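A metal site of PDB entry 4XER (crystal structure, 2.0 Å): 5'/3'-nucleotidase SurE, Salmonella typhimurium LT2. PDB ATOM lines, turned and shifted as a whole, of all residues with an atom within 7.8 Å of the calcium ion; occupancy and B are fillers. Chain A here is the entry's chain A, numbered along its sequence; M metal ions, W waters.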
ATOM      1  N   ASN A  21      27.824 -33.135  -0.492  1.00  0.00           N
ATOM      2  CA  ASN A  21      27.375 -32.232   0.554  1.00  0.00           C
ATOM      3  C   ASN A  21      28.567 -31.652   1.297  1.00  0.00           C
ATOM      4  O   ASN A  21      29.674 -32.065   1.083  1.00  0.00           O
ATOM      5  CB  ASN A  21      26.477 -32.951   1.577  1.00  0.00           C
ATOM      6  CG  ASN A  21      27.240 -33.792   2.600  1.00  0.00           C
ATOM      7  OD1 ASN A  21      28.409 -34.061   2.479  1.00  0.00           O
ATOM      8  ND2 ASN A  21      26.544 -34.200   3.604  1.00  0.00           N
ATOM      9  N   ASP A  22      28.339 -30.688   2.151  1.00  0.00           N
ATOM     10  CA  ASP A  22      29.458 -30.349   3.037  1.00  0.00           C
ATOM     11  C   ASP A  22      29.431 -30.871   4.441  1.00  0.00           C
ATOM     12  O   ASP A  22      30.399 -30.685   5.186  1.00  0.00           O
ATOM     13  CB  ASP A  22      29.711 -28.838   2.948  1.00  0.00           C
ATOM     14  CG  ASP A  22      28.801 -28.064   3.765  1.00  0.00           C
ATOM     15  OD1 ASP A  22      27.797 -28.602   4.252  1.00  0.00           O
ATOM     16  OD2 ASP A  22      29.085 -26.874   3.897  1.00  0.00           O
ATOM     17  N   ASP A  23      28.331 -31.522   4.809  1.00  0.00           N
ATOM     18  CA  ASP A  23      28.172 -32.077   6.143  1.00  0.00           C
ATOM     19  C   ASP A  23      28.842 -33.429   6.262  1.00  0.00           C
ATOM     20  O   ASP A  23      28.906 -34.004   7.357  1.00  0.00           O
ATOM     21  CB  ASP A  23      26.686 -32.189   6.505  1.00  0.00           C
ATOM     22  CG  ASP A  23      26.042 -30.835   6.734  1.00  0.00           C
ATOM     23  OD1 ASP A  23      26.773 -29.873   7.052  1.00  0.00           O
ATOM     24  OD2 ASP A  23      24.808 -30.744   6.606  1.00  0.00           O
ATOM     25  N   GLY A  24      29.347 -33.964   5.152  1.00  0.00           N
ATOM     26  CA  GLY A  24      30.000 -35.271   5.196  1.00  0.00           C
ATOM     27  C   GLY A  24      29.106 -36.490   4.926  1.00  0.00           C
ATOM     28  O   GLY A  24      27.918 -36.392   5.093  1.00  0.00           O
ATOM     29  N   ASN A  51      32.246 -33.439   8.738  1.00  0.00           N
ATOM     30  CA  ASN A  51      31.622 -32.128   8.590  1.00  0.00           C
ATOM     31  C   ASN A  51      32.601 -30.966   8.233  1.00  0.00           C
ATOM     32  O   ASN A  51      33.584 -30.718   8.873  1.00  0.00           O
ATOM     33  CB  ASN A  51      30.782 -31.771   9.790  1.00  0.00           C
ATOM     34  CG  ASN A  51      29.699 -30.768   9.459  1.00  0.00           C
ATOM     35  OD1 ASN A  51      29.911 -29.774   8.726  1.00  0.00           O
ATOM     36  ND2 ASN A  51      28.486 -31.053   9.951  1.00  0.00           N
ATOM     37  N   ARG A  52      32.315 -30.289   7.141  1.00  0.00           N
ATOM     38  CA  ARG A  52      33.258 -29.318   6.547  1.00  0.00           C
ATOM     39  C   ARG A  52      32.512 -28.016   6.298  1.00  0.00           C
ATOM     40  O   ARG A  52      32.811 -27.288   5.353  1.00  0.00           O
ATOM     41  CB  ARG A  52      33.843 -29.829   5.196  1.00  0.00           C
ATOM     42  CG  ARG A  52      34.891 -30.962   5.220  1.00  0.00           C
ATOM     43  CD  ARG A  52      36.062 -30.676   6.174  1.00  0.00           C
ATOM     44  NE  ARG A  52      36.872 -29.584   5.654  1.00  0.00           N
ATOM     45  CZ  ARG A  52      38.040 -29.712   5.014  1.00  0.00           C
ATOM     46  NH1 ARG A  52      38.607 -30.888   4.817  1.00  0.00           N
ATOM     47  NH2 ARG A  52      38.676 -28.614   4.609  1.00  0.00           N
ATOM     48  N   SER A  53      31.487 -27.767   7.105  1.00  0.00           N
ATOM     49  CA  SER A  53      30.728 -26.458   7.027  1.00  0.00           C
ATOM     50  C   SER A  53      31.725 -25.270   7.204  1.00  0.00           C
ATOM     51  O   SER A  53      32.700 -25.317   7.968  1.00  0.00           O
ATOM     52  CB  SER A  53      29.545 -26.445   8.004  1.00  0.00           C
ATOM     53  OG  SER A  53      28.702 -27.640   7.874  1.00  0.00           O
ATOM     54  N   GLY A  54      31.635 -24.219   6.464  1.00  0.00           N
ATOM     55  CA  GLY A  54      32.900 -23.416   6.620  1.00  0.00           C
ATOM     56  C   GLY A  54      33.922 -23.679   5.515  1.00  0.00           C
ATOM     57  O   GLY A  54      34.718 -22.784   5.231  1.00  0.00           O
ATOM     58  N   ALA A  55      33.860 -24.853   4.806  1.00  0.00           N
ATOM     59  CA  ALA A  55      34.879 -25.159   3.745  1.00  0.00           C
ATOM     60  C   ALA A  55      34.668 -24.257   2.590  1.00  0.00           C
ATOM     61  O   ALA A  55      35.603 -23.956   1.846  1.00  0.00           O
ATOM     62  CB  ALA A  55      34.843 -26.651   3.323  1.00  0.00           C
ATOM     63  N   ILE A 105      21.136 -32.886   1.496  1.00  0.00           N
ATOM     64  CA  ILE A 105      20.427 -31.704   1.976  1.00  0.00           C
ATOM     65  C   ILE A 105      21.266 -31.083   3.126  1.00  0.00           C
ATOM     66  O   ILE A 105      21.578 -31.764   4.067  1.00  0.00           O
ATOM     67  CB  ILE A 105      19.047 -32.133   2.588  1.00  0.00           C
ATOM     68  CG1 ILE A 105      18.174 -32.791   1.476  1.00  0.00           C
ATOM     69  CG2 ILE A 105      18.314 -30.848   3.086  1.00  0.00           C
ATOM     70  CD1 ILE A 105      17.221 -33.830   2.054  1.00  0.00           C
ATOM     71  N   ASN A 106      21.618 -29.815   3.041  1.00  0.00           N
ATOM     72  CA  ASN A 106      22.350 -29.202   4.135  1.00  0.00           C
ATOM     73  C   ASN A 106      21.426 -29.015   5.385  1.00  0.00           C
ATOM     74  O   ASN A 106      20.263 -28.624   5.250  1.00  0.00           O
ATOM     75  CB  ASN A 106      22.842 -27.839   3.728  1.00  0.00           C
ATOM     76  CG  ASN A 106      23.830 -27.249   4.774  1.00  0.00           C
ATOM     77  OD1 ASN A 106      24.870 -27.845   5.011  1.00  0.00           O
ATOM     78  ND2 ASN A 106      23.519 -26.079   5.366  1.00  0.00           N
ATOM     79  N   ALA A 107      21.989 -29.210   6.574  1.00  0.00           N
ATOM     80  CA  ALA A 107      21.337 -28.872   7.875  1.00  0.00           C
ATOM     81  C   ALA A 107      21.469 -27.376   8.072  1.00  0.00           C
ATOM     82  O   ALA A 107      22.493 -26.878   8.539  1.00  0.00           O
ATOM     83  CB  ALA A 107      22.056 -29.604   8.994  1.00  0.00           C
ATOM     84  N   GLY A 108      20.474 -26.633   7.612  1.00  0.00           N
ATOM     85  CA  GLY A 108      20.449 -25.214   7.814  1.00  0.00           C
ATOM     86  C   GLY A 108      20.487 -24.506   6.491  1.00  0.00           C
ATOM     87  O   GLY A 108      20.965 -25.086   5.455  1.00  0.00           O
ATOM     88  N   PRO A 109      20.020 -23.248   6.499  1.00  0.00           N
ATOM     89  CA  PRO A 109      19.796 -22.542   5.242  1.00  0.00           C
ATOM     90  C   PRO A 109      21.084 -21.992   4.626  1.00  0.00           C
ATOM     91  O   PRO A 109      22.097 -21.787   5.308  1.00  0.00           O
ATOM     92  CB  PRO A 109      18.836 -21.416   5.685  1.00  0.00           C
ATOM     93  CG  PRO A 109      19.378 -21.063   7.064  1.00  0.00           C
ATOM     94  CD  PRO A 109      19.563 -22.425   7.663  1.00  0.00           C
ATOM     95  N   ASN A 110      21.054 -21.731   3.329  1.00  0.00           N
ATOM     96  CA  ASN A 110      22.090 -21.121   2.635  1.00  0.00           C
ATOM     97  C   ASN A 110      21.473 -20.007   1.830  1.00  0.00           C
ATOM     98  O   ASN A 110      21.088 -20.134   0.651  1.00  0.00           O
ATOM     99  CB  ASN A 110      22.924 -22.138   1.776  1.00  0.00           C
ATOM    100  CG  ASN A 110      23.869 -22.930   2.625  1.00  0.00           C
ATOM    101  OD1 ASN A 110      23.692 -24.122   2.828  1.00  0.00           O
ATOM    102  ND2 ASN A 110      24.827 -22.255   3.205  1.00  0.00           N
ATOM    103  N   SER A 118      29.240 -21.039   1.343  1.00  0.00           N
ATOM    104  CA  SER A 118      28.581 -22.306   1.637  1.00  0.00           C
ATOM    105  C   SER A 118      29.339 -23.455   0.887  1.00  0.00           C
ATOM    106  O   SER A 118      29.568 -23.320  -0.340  1.00  0.00           O
ATOM    107  CB  SER A 118      27.164 -22.253   0.989  1.00  0.00           C
ATOM    108  OG  SER A 118      26.540 -23.539   1.085  1.00  0.00           O
ATOM    109  N   GLY A 119      29.673 -24.517   1.609  1.00  0.00           N
ATOM    110  CA  GLY A 119      30.322 -25.684   1.003  1.00  0.00           C
ATOM    111  C   GLY A 119      29.244 -26.484   0.196  1.00  0.00           C
ATOM    112  O   GLY A 119      29.571 -27.048  -0.841  1.00  0.00           O
ATOM    113  N   THR A 120      28.011 -26.494   0.695  1.00  0.00           N
ATOM    114  CA  THR A 120      26.858 -27.021  -0.073  1.00  0.00           C
ATOM    115  C   THR A 120      26.787 -26.417  -1.460  1.00  0.00           C
ATOM    116  O   THR A 120      26.738 -27.164  -2.437  1.00  0.00           O
ATOM    117  CB  THR A 120      25.539 -26.802   0.638  1.00  0.00           C
ATOM    118  OG1 THR A 120      25.636 -27.523   1.893  1.00  0.00           O
ATOM    119  CG2 THR A 120      24.317 -27.509  -0.173  1.00  0.00           C
ATOM    120  N   SER A 138      19.167 -26.973   0.705  1.00  0.00           N
ATOM    121  CA  SER A 138      19.417 -26.746   2.136  1.00  0.00           C
ATOM    122  C   SER A 138      18.092 -26.596   2.818  1.00  0.00           C
ATOM    123  O   SER A 138      17.141 -26.037   2.245  1.00  0.00           O
ATOM    124  CB  SER A 138      20.217 -25.447   2.332  1.00  0.00           C
ATOM    125  OG  SER A 138      21.377 -25.414   1.577  1.00  0.00           O
HETATM  126 CA    CA M   1      26.776 -27.620   6.298  1.00  0.00          CA
HETATM  127  O   HOH W   1      27.336 -25.512   6.013  1.00  0.00           O
HETATM  128  O   HOH W   2      25.346 -27.829   8.116  1.00  0.00           O
HETATM  129  O   HOH W   3      25.310 -25.435   7.939  1.00  0.00           O
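The side-chain amide oxygen of Asn 106 sits close to the side-chain hydroxyl of Thr 120, at 3.2 Å.
The side-chain amide nitrogen of Asn 106 sits at hydrogen-bond distance from the side-chain amide oxygen of Asn 110, 3.2 Å away.
ND2 of Asn 106 is in hydrogen-bond range of O of Gly 108, 2.7 Å away.
The side-chain carboxylate of Asp 23 lies within hydrogen-bond range of the backbone NH of Ala 107, at 3.2 Å.
ND2 of Asn 21 sits close to N of Asp 23 (3.4 Å).
The side-chain carboxylate of Asp 22 lies within hydrogen-bond range of the backbone NH of Thr 120.
The backbone carbonyl oxygen of Asp 22 sits at hydrogen-bond distance from the backbone NH of Arg 52 (2.8 Å).
OD2 of Asp 22 lies within hydrogen-bond range of N of Gly 119, at 3.3 Å.
Within 4 Å of the calcium ion: Asp 22, Asp 23, Ser 53 and Asn 106.
Along chain A the residues within 4 Å of the calcium ion span positions 22 to 106.
The nearest printed residue that does not touch the calcium ion is Asn 51 (4.5 Å).
Water W1 binds the calcium ion (2.2 Å).
The calcium ion is bound by OD1 of Asn 106 (2.3 Å).
Water W2 is bound to the calcium ion.
The side-chain carboxylate (OD1) of Asp 23 binds the calcium ion (2.4 Å).
The calcium ion is bound by OD1 of Asp 22 (2.5 Å).
The side-chain hydroxyl (OG) of Ser 53 is bound to the calcium ion, 2.5 Å away.
The calcium ion has six donor atoms within binding distance.
Slightly farther from the calcium ion lies water W3 (3.1 Å).
Water W2 bridges the backbone carbonyl oxygen of Ala 107 (3.0 Å) and the side-chain carboxylate of Asp 23 (3.3 Å).
Water W3 lies within hydrogen-bond range of the side-chain amide nitrogen of Asn 106 (3.2 Å) and the backbone carbonyl oxygen of Ala 107 (3.2 Å).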
